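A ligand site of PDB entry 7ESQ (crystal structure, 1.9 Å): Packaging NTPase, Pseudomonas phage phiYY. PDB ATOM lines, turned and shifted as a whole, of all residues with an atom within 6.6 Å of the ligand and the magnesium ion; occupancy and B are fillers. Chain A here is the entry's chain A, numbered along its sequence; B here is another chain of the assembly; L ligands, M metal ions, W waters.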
ATOM      1  N   GLY A 144       5.520   6.379 -10.503  1.00  0.00           N
ATOM      2  CA  GLY A 144       5.336   5.223  -9.639  1.00  0.00           C
ATOM      3  C   GLY A 144       4.899   5.655  -8.250  1.00  0.00           C
ATOM      4  O   GLY A 144       4.954   6.829  -7.882  1.00  0.00           O
ATOM      5  N   GLY A 145       4.460   4.674  -7.461  1.00  0.00           N
ATOM      6  CA  GLY A 145       3.873   4.966  -6.164  1.00  0.00           C
ATOM      7  C   GLY A 145       4.910   5.254  -5.090  1.00  0.00           C
ATOM      8  O   GLY A 145       6.108   5.360  -5.342  1.00  0.00           O
ATOM      9  N   THR A 146       4.424   5.385  -3.856  1.00  0.00           N
ATOM     10  CA  THR A 146       5.303   5.676  -2.736  1.00  0.00           C
ATOM     11  C   THR A 146       6.297   4.534  -2.514  1.00  0.00           C
ATOM     12  O   THR A 146       5.924   3.359  -2.460  1.00  0.00           O
ATOM     13  CB  THR A 146       4.442   5.905  -1.494  1.00  0.00           C
ATOM     14  OG1 THR A 146       3.622   7.047  -1.736  1.00  0.00           O
ATOM     15  CG2 THR A 146       5.298   6.110  -0.259  1.00  0.00           C
ATOM     16  N   GLY A 147       7.574   4.885  -2.403  1.00  0.00           N
ATOM     17  CA  GLY A 147       8.634   3.901  -2.244  1.00  0.00           C
ATOM     18  C   GLY A 147       8.848   2.994  -3.430  1.00  0.00           C
ATOM     19  O   GLY A 147       9.424   1.912  -3.277  1.00  0.00           O
ATOM     20  N   ALA A 148       8.434   3.401  -4.632  1.00  0.00           N
ATOM     21  CA  ALA A 148       8.646   2.571  -5.822  1.00  0.00           C
ATOM     22  C   ALA A 148      10.092   2.570  -6.290  1.00  0.00           C
ATOM     23  O   ALA A 148      10.416   1.821  -7.212  1.00  0.00           O
ATOM     24  CB  ALA A 148       7.747   3.044  -6.965  1.00  0.00           C
ATOM     25  N   GLY A 149      10.960   3.381  -5.692  1.00  0.00           N
ATOM     26  CA  GLY A 149      12.344   3.469  -6.121  1.00  0.00           C
ATOM     27  C   GLY A 149      12.644   4.550  -7.134  1.00  0.00           C
ATOM     28  O   GLY A 149      13.682   4.468  -7.809  1.00  0.00           O
ATOM     29  N   LYS A 150      11.787   5.564  -7.257  1.00  0.00           N
ATOM     30  CA  LYS A 150      12.000   6.627  -8.248  1.00  0.00           C
ATOM     31  C   LYS A 150      13.247   7.447  -7.931  1.00  0.00           C
ATOM     32  O   LYS A 150      14.081   7.720  -8.813  1.00  0.00           O
ATOM     33  CB  LYS A 150      10.763   7.527  -8.312  1.00  0.00           C
ATOM     34  CG  LYS A 150       9.483   6.826  -8.722  1.00  0.00           C
ATOM     35  CD  LYS A 150       8.291   7.806  -8.793  1.00  0.00           C
ATOM     36  CE  LYS A 150       8.014   8.477  -7.452  1.00  0.00           C
ATOM     37  NZ  LYS A 150       7.627   7.494  -6.364  1.00  0.00           N
ATOM     38  N   SER A 151      13.413   7.860  -6.668  1.00  0.00           N
ATOM     39  CA  SER A 151      14.587   8.659  -6.334  1.00  0.00           C
ATOM     40  C   SER A 151      15.887   7.902  -6.574  1.00  0.00           C
ATOM     41  O   SER A 151      16.877   8.464  -7.068  1.00  0.00           O
ATOM     42  CB  SER A 151      14.528   9.138  -4.876  1.00  0.00           C
ATOM     43  OG  SER A 151      13.477  10.063  -4.636  1.00  0.00           O
ATOM     44  N   SER A 152      15.935   6.623  -6.192  1.00  0.00           N
ATOM     45  CA  SER A 152      17.186   5.894  -6.418  1.00  0.00           C
ATOM     46  C   SER A 152      17.375   5.530  -7.889  1.00  0.00           C
ATOM     47  O   SER A 152      18.522   5.383  -8.334  1.00  0.00           O
ATOM     48  CB  SER A 152      17.244   4.625  -5.544  1.00  0.00           C
ATOM     49  OG  SER A 152      16.264   3.706  -5.983  1.00  0.00           O
ATOM     50  N   ARG A 164      16.436  18.908  -6.072  1.00  0.00           N
ATOM     51  CA  ARG A 164      15.553  18.373  -5.045  1.00  0.00           C
ATOM     52  C   ARG A 164      14.512  19.417  -4.661  1.00  0.00           C
ATOM     53  O   ARG A 164      14.858  20.522  -4.243  1.00  0.00           O
ATOM     54  CB  ARG A 164      16.362  17.911  -3.831  1.00  0.00           C
ATOM     55  CG  ARG A 164      17.255  16.701  -4.175  1.00  0.00           C
ATOM     56  CD  ARG A 164      16.443  15.407  -4.034  1.00  0.00           C
ATOM     57  NE  ARG A 164      16.175  15.139  -2.615  1.00  0.00           N
ATOM     58  CZ  ARG A 164      15.240  14.296  -2.182  1.00  0.00           C
ATOM     59  NH1 ARG A 164      14.504  13.609  -3.043  1.00  0.00           N
ATOM     60  NH2 ARG A 164      15.062  14.118  -0.883  1.00  0.00           N
ATOM     61  N   GLU A 167      10.454  17.430  -1.469  1.00  0.00           N
ATOM     62  CA  GLU A 167      10.662  16.129  -0.869  1.00  0.00           C
ATOM     63  C   GLU A 167      11.362  16.293   0.480  1.00  0.00           C
ATOM     64  O   GLU A 167      12.134  17.239   0.659  1.00  0.00           O
ATOM     65  CB  GLU A 167      11.540  15.245  -1.771  1.00  0.00           C
ATOM     66  CG  GLU A 167      10.874  14.833  -3.115  1.00  0.00           C
ATOM     67  CD  GLU A 167       9.754  13.800  -2.950  1.00  0.00           C
ATOM     68  OE1 GLU A 167       8.803  13.821  -3.765  1.00  0.00           O
ATOM     69  OE2 GLU A 167       9.755  13.036  -1.966  1.00  0.00           O
ATOM     70  N   PRO A 168      11.146  15.378   1.435  1.00  0.00           N
ATOM     71  CA  PRO A 168      11.824  15.495   2.736  1.00  0.00           C
ATOM     72  C   PRO A 168      13.309  15.260   2.603  1.00  0.00           C
ATOM     73  O   PRO A 168      13.768  14.542   1.715  1.00  0.00           O
ATOM     74  CB  PRO A 168      11.173  14.385   3.577  1.00  0.00           C
ATOM     75  CG  PRO A 168      10.813  13.326   2.531  1.00  0.00           C
ATOM     76  CD  PRO A 168      10.350  14.131   1.329  1.00  0.00           C
ATOM     77  N   GLU A 170      16.627  13.609   2.823  1.00  0.00           N
ATOM     78  CA  GLU A 170      16.902  12.171   2.758  1.00  0.00           C
ATOM     79  C   GLU A 170      18.401  11.963   2.657  1.00  0.00           C
ATOM     80  O   GLU A 170      19.178  12.921   2.603  1.00  0.00           O
ATOM     81  CB  GLU A 170      16.199  11.517   1.561  1.00  0.00           C
ATOM     82  CG  GLU A 170      14.685  11.304   1.742  1.00  0.00           C
ATOM     83  CD  GLU A 170      13.981  10.958   0.429  1.00  0.00           C
ATOM     84  OE1 GLU A 170      13.870   9.746   0.129  1.00  0.00           O
ATOM     85  OE2 GLU A 170      13.477  11.877  -0.270  1.00  0.00           O
ATOM     86  N   PHE A 172      19.811  11.121   0.050  1.00  0.00           N
ATOM     87  CA  PHE A 172      20.206  11.703  -1.239  1.00  0.00           C
ATOM     88  C   PHE A 172      20.753  13.117  -1.074  1.00  0.00           C
ATOM     89  O   PHE A 172      21.625  13.541  -1.843  1.00  0.00           O
ATOM     90  CB  PHE A 172      19.012  11.721  -2.207  1.00  0.00           C
ATOM     91  CG  PHE A 172      18.297  10.399  -2.318  1.00  0.00           C
ATOM     92  CD1 PHE A 172      18.887   9.317  -2.958  1.00  0.00           C
ATOM     93  CD2 PHE A 172      17.019  10.241  -1.777  1.00  0.00           C
ATOM     94  CE1 PHE A 172      18.233   8.100  -3.058  1.00  0.00           C
ATOM     95  CE2 PHE A 172      16.366   9.018  -1.869  1.00  0.00           C
ATOM     96  CZ  PHE A 172      16.973   7.950  -2.513  1.00  0.00           C
ATOM     97  N   ASP A 204      13.522  16.095  -8.676  1.00  0.00           N
ATOM     98  CA  ASP A 204      12.920  15.163  -7.727  1.00  0.00           C
ATOM     99  C   ASP A 204      12.343  16.049  -6.628  1.00  0.00           C
ATOM    100  O   ASP A 204      13.075  16.388  -5.696  1.00  0.00           O
ATOM    101  CB  ASP A 204      13.993  14.184  -7.169  1.00  0.00           C
ATOM    102  CG  ASP A 204      13.393  13.041  -6.335  1.00  0.00           C
ATOM    103  OD1 ASP A 204      12.153  12.892  -6.290  1.00  0.00           O
ATOM    104  OD2 ASP A 204      14.181  12.300  -5.708  1.00  0.00           O
ATOM    105  N   SER A 205      11.071  16.432  -6.724  1.00  0.00           N
ATOM    106  CA  SER A 205      10.081  15.862  -7.642  1.00  0.00           C
ATOM    107  C   SER A 205       9.013  16.914  -7.989  1.00  0.00           C
ATOM    108  O   SER A 205       9.101  18.051  -7.502  1.00  0.00           O
ATOM    109  CB  SER A 205       9.422  14.655  -7.003  1.00  0.00           C
ATOM    110  OG  SER A 205       8.554  15.129  -5.964  1.00  0.00           O
ATOM    111  N   ARG A 207       6.051  16.572  -6.817  1.00  0.00           N
ATOM    112  CA  ARG A 207       5.063  16.281  -5.777  1.00  0.00           C
ATOM    113  C   ARG A 207       4.070  17.424  -5.589  1.00  0.00           C
ATOM    114  O   ARG A 207       2.859  17.211  -5.497  1.00  0.00           O
ATOM    115  CB  ARG A 207       5.821  16.005  -4.475  1.00  0.00           C
ATOM    116  CG  ARG A 207       5.018  15.533  -3.254  1.00  0.00           C
ATOM    117  CD  ARG A 207       6.047  14.883  -2.304  1.00  0.00           C
ATOM    118  NE  ARG A 207       5.803  15.070  -0.876  1.00  0.00           N
ATOM    119  CZ  ARG A 207       5.097  14.225  -0.126  1.00  0.00           C
ATOM    120  NH1 ARG A 207       4.943  14.484   1.169  1.00  0.00           N
ATOM    121  NH2 ARG A 207       4.568  13.135  -0.652  1.00  0.00           N
ATOM    122  N   VAL A 247      10.578  13.361 -11.636  1.00  0.00           N
ATOM    123  CA  VAL A 247       9.900  12.352 -10.828  1.00  0.00           C
ATOM    124  C   VAL A 247       8.481  12.807 -10.504  1.00  0.00           C
ATOM    125  O   VAL A 247       8.260  13.960 -10.121  1.00  0.00           O
ATOM    126  CB  VAL A 247      10.692  12.098  -9.525  1.00  0.00           C
ATOM    127  CG1 VAL A 247       9.895  11.199  -8.578  1.00  0.00           C
ATOM    128  CG2 VAL A 247      12.070  11.527  -9.833  1.00  0.00           C
ATOM    129  N   VAL A 248       7.511  11.906 -10.649  1.00  0.00           N
ATOM    130  CA  VAL A 248       6.115  12.192 -10.282  1.00  0.00           C
ATOM    131  C   VAL A 248       5.543  10.980  -9.570  1.00  0.00           C
ATOM    132  O   VAL A 248       5.491   9.889 -10.153  1.00  0.00           O
ATOM    133  CB  VAL A 248       5.229  12.528 -11.496  1.00  0.00           C
ATOM    134  CG1 VAL A 248       3.846  12.998 -11.025  1.00  0.00           C
ATOM    135  CG2 VAL A 248       5.868  13.570 -12.389  1.00  0.00           C
ATOM    136  N   ASN A 249       5.057  11.164  -8.345  1.00  0.00           N
ATOM    137  CA  ASN A 249       4.236  10.178  -7.642  1.00  0.00           C
ATOM    138  C   ASN A 249       2.805  10.675  -7.718  1.00  0.00           C
ATOM    139  O   ASN A 249       2.426  11.590  -6.978  1.00  0.00           O
ATOM    140  CB  ASN A 249       4.699  10.041  -6.182  1.00  0.00           C
ATOM    141  CG  ASN A 249       3.878   9.024  -5.375  1.00  0.00           C
ATOM    142  OD1 ASN A 249       2.764   8.649  -5.741  1.00  0.00           O
ATOM    143  ND2 ASN A 249       4.447   8.564  -4.246  1.00  0.00           N
ATOM    144  N   MET A 251      -0.112   9.409  -6.868  1.00  0.00           N
ATOM    145  CA  MET A 251      -1.049   9.061  -5.790  1.00  0.00           C
ATOM    146  C   MET A 251      -2.332   8.450  -6.359  1.00  0.00           C
ATOM    147  O   MET A 251      -3.427   8.710  -5.883  1.00  0.00           O
ATOM    148  CB  MET A 251      -1.372  10.275  -4.924  1.00  0.00           C
ATOM    149  CG  MET A 251      -0.173  10.900  -4.180  1.00  0.00           C
ATOM    150  SD  MET A 251       0.264   9.945  -2.722  1.00  0.00           S
ATOM    151  CE  MET A 251       2.009  10.255  -2.509  1.00  0.00           C
ATOM    152  N   LEU A 274       8.109   2.871 -12.512  1.00  0.00           N
ATOM    153  CA  LEU A 274       8.810   2.021 -11.552  1.00  0.00           C
ATOM    154  C   LEU A 274       7.800   1.300 -10.669  1.00  0.00           C
ATOM    155  O   LEU A 274       6.793   1.878 -10.234  1.00  0.00           O
ATOM    156  CB  LEU A 274       9.768   2.834 -10.683  1.00  0.00           C
ATOM    157  CG  LEU A 274      11.183   3.216 -11.101  1.00  0.00           C
ATOM    158  CD1 LEU A 274      12.039   1.952 -11.239  1.00  0.00           C
ATOM    159  CD2 LEU A 274      11.098   3.854 -12.468  1.00  0.00           C
ATOM    160  N   ASN B 263       2.377   6.840   3.477  1.00  0.00           N
ATOM    161  CA  ASN B 263       2.572   8.150   2.873  1.00  0.00           C
ATOM    162  C   ASN B 263       3.031   9.184   3.888  1.00  0.00           C
ATOM    163  O   ASN B 263       3.777  10.099   3.534  1.00  0.00           O
ATOM    164  CB  ASN B 263       1.287   8.607   2.186  1.00  0.00           C
ATOM    165  CG  ASN B 263       0.956   7.743   0.971  1.00  0.00           C
ATOM    166  OD1 ASN B 263       1.832   7.063   0.433  1.00  0.00           O
ATOM    167  ND2 ASN B 263      -0.296   7.773   0.544  1.00  0.00           N
ATOM    168  N   ALA B 266       6.678   8.536   4.372  1.00  0.00           N
ATOM    169  CA  ALA B 266       7.417   9.014   3.215  1.00  0.00           C
ATOM    170  C   ALA B 266       7.547  10.531   3.178  1.00  0.00           C
ATOM    171  O   ALA B 266       8.267  11.062   2.321  1.00  0.00           O
ATOM    172  CB  ALA B 266       6.764   8.521   1.921  1.00  0.00           C
ATOM    173  N   SER B 267       6.868  11.257   4.074  1.00  0.00           N
ATOM    174  CA  SER B 267       6.894  12.705   4.085  1.00  0.00           C
ATOM    175  C   SER B 267       7.845  13.306   5.109  1.00  0.00           C
ATOM    176  O   SER B 267       8.015  14.526   5.102  1.00  0.00           O
ATOM    177  CB  SER B 267       5.486  13.271   4.342  1.00  0.00           C
ATOM    178  OG  SER B 267       4.521  12.660   3.491  1.00  0.00           O
ATOM    179  N   ARG B 285      14.561   7.362   8.981  1.00  0.00           N
ATOM    180  CA  ARG B 285      15.630   7.607   8.023  1.00  0.00           C
ATOM    181  C   ARG B 285      16.864   8.019   8.800  1.00  0.00           C
ATOM    182  O   ARG B 285      16.801   8.935   9.630  1.00  0.00           O
ATOM    183  CB  ARG B 285      15.253   8.716   7.050  1.00  0.00           C
ATOM    184  CG  ARG B 285      14.048   8.459   6.187  1.00  0.00           C
ATOM    185  CD  ARG B 285      13.887   9.596   5.197  1.00  0.00           C
ATOM    186  NE  ARG B 285      12.490   9.935   5.004  1.00  0.00           N
ATOM    187  CZ  ARG B 285      11.744   9.523   3.990  1.00  0.00           C
ATOM    188  NH1 ARG B 285      12.258   8.736   3.054  1.00  0.00           N
ATOM    189  NH2 ARG B 285      10.479   9.881   3.913  1.00  0.00           N
ATOM    190  N   ARG B 290      18.187   3.653   6.485  1.00  0.00           N
ATOM    191  CA  ARG B 290      16.771   3.843   6.792  1.00  0.00           C
ATOM    192  C   ARG B 290      16.360   2.662   7.663  1.00  0.00           C
ATOM    193  O   ARG B 290      16.405   1.516   7.203  1.00  0.00           O
ATOM    194  CB  ARG B 290      15.897   3.865   5.521  1.00  0.00           C
ATOM    195  CG  ARG B 290      14.413   4.151   5.835  1.00  0.00           C
ATOM    196  CD  ARG B 290      13.459   4.201   4.608  1.00  0.00           C
ATOM    197  NE  ARG B 290      13.636   5.282   3.636  1.00  0.00           N
ATOM    198  CZ  ARG B 290      12.992   5.334   2.476  1.00  0.00           C
ATOM    199  NH1 ARG B 290      12.085   4.405   2.173  1.00  0.00           N
ATOM    200  NH2 ARG B 290      13.214   6.329   1.621  1.00  0.00           N
HETATM  201  O1  LIG L   1      11.273   7.905  -4.600  1.00  0.00           O
HETATM  202  P1  LIG L   1      10.385   6.713  -4.344  1.00  0.00           P
HETATM  203  O2  LIG L   1       9.761   6.185  -5.592  1.00  0.00           O
HETATM  204  O3  LIG L   1      11.253   5.650  -3.712  1.00  0.00           O
HETATM  205  O4  LIG L   1       9.163   7.045  -3.298  1.00  0.00           O
HETATM  206  P2  LIG L   1       8.581   8.546  -2.929  1.00  0.00           P
HETATM  207  O5  LIG L   1       9.754   9.470  -2.738  1.00  0.00           O
HETATM  208  O6  LIG L   1       7.818   8.366  -1.637  1.00  0.00           O
HETATM  209  O7  LIG L   1       7.654   9.007  -4.027  1.00  0.00           O
HETATM  210 MG    MG M   1      11.632   9.671  -3.598  1.00  0.00          MG
HETATM  211  O   HOH W   1      12.065  11.404  -2.415  1.00  0.00           O
HETATM  212  O   HOH W   2      13.992   5.723  -4.201  1.00  0.00           O
HETATM  213  O   HOH W   3      12.701   8.706  -2.032  1.00  0.00           O
HETATM  214  O   HOH W   4      11.769   6.251  -1.091  1.00  0.00           O
HETATM  215  O   HOH W   5       5.486   9.678  -1.092  1.00  0.00           O
HETATM  216  O   HOH W   6      10.468   9.571   0.527  1.00  0.00           O
HETATM  217  O   HOH W   7      10.730  11.008  -5.071  1.00  0.00           O
HETATM  218  O   HOH W   8       9.493   6.891   0.031  1.00  0.00           O
HETATM  219  O   HOH W   9       7.756  11.584  -4.708  1.00  0.00           O
HETATM  220  O   HOH W  10       8.287  11.464  -0.509  1.00  0.00           O
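OG of Ser 151 lies close to OD2 of Asp 204 (2.6 Å).
The side-chain amino group of Lys 150 sits at hydrogen-bond distance from the backbone carbonyl oxygen of Gly 145, 2.8 Å away.
The backbone carbonyl oxygen (O) of Gly 149 is in hydrogen-bond range of the side-chain hydroxyl (OG) of Ser 152.
The side-chain amide nitrogen (ND2) of Asn 249 lies within hydrogen-bond range of the side-chain hydroxyl (OG1) of Thr 146, 3.0 Å away.
The side-chain amide oxygen (OD1) of Asn 249 sits at hydrogen-bond distance from the backbone NH (N) of Met 251 (3.2 Å).
OG of Ser 205 sits at hydrogen-bond distance from OE1 of Glu 167 (2.6 Å).
OD1 of Asn 263 of chain B is in hydrogen-bond range of OG1 of Thr 146 (2.8 Å).
The guanidinium group (NH2) of Arg 285 of chain B sits at hydrogen-bond distance from the backbone carbonyl oxygen (O) of Ala 266 of chain B.
Within 4 Å of the magnesium ion: Ser 151.
Residues that only touch the ligand: Gly 145, Thr 146, Glu 167 and Ala 266 of chain B.
Hydrophobic or aromatic side chains within 4 Å of the ligand: Ala 148 and Ala 266 of chain B.
Within 4 Å of the ligand: Gly 145, Thr 146, Gly 147, Ala 148, Gly 149, Lys 150, Ser 151, Glu 167, Asn 249 and Ala 266 of chain B.
The nearest printed residue that does not touch the ligand is Glu 170 (5.0 Å).
The magnesium ion is bound by an oxygen (O1) of the ligand (2.1 Å), an oxygen (O5) of the ligand (2.1 Å), water W3 (2.1 Å), water W1 (2.1 Å), the side-chain hydroxyl (OG) of Ser 151 (2.2 Å) and water W7 (2.2 Å).
The magnesium ion has six donor atoms within binding distance.
Water W1 lies within hydrogen-bond range of the side-chain carboxylate of Glu 170, the side-chain carboxylate of Glu 167 and the guanidinium group of Arg 164.
Water W9 bridges OE1 of Glu 167 (2.6 Å) and O7 of the ligand (2.7 Å).
Water W4 bridges O3 of the ligand (2.7 Å) and NH2 of Arg 290 of chain B (3.1 Å).
Water W2 lies within hydrogen-bond range of an oxygen (O3) of the ligand (2.8 Å), the backbone NH (N) of Ser 152 (2.9 Å) and the backbone NH (N) of Ser 151 (3.3 Å).
Water W10 lies within hydrogen-bond range of the side-chain carboxylate of Glu 167 (2.6 Å), the backbone carbonyl oxygen of Ala 266 of chain B (2.9 Å) and an oxygen (O6) of the ligand (3.3 Å).
Water W6 lies within hydrogen-bond range of O of Ala 266 of chain B, NH1 of Arg 285 of chain B and OE1 of Glu 170.
O1 of the ligand sits close to N of Ser 151, 3.0 Å away.
An oxygen (O2) of the ligand sits at hydrogen-bond distance from the backbone NH (N) of Lys 150, at 2.7 Å.
An oxygen (O2) of the ligand lies within salt-bridge range of the side-chain amino group of Lys 150, 2.6 Å away.
An oxygen (O4) of the ligand sits at hydrogen-bond distance from the backbone NH (N) of Gly 147 (2.8 Å).
O3 of the ligand lies within hydrogen-bond range of N of Gly 149.
An oxygen (O2) of the ligand lies within hydrogen-bond range of the backbone NH (N) of Ala 148, at 3.2 Å.
ND2 of Asn 249 is in hydrogen-bond range of O7 of the ligand.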
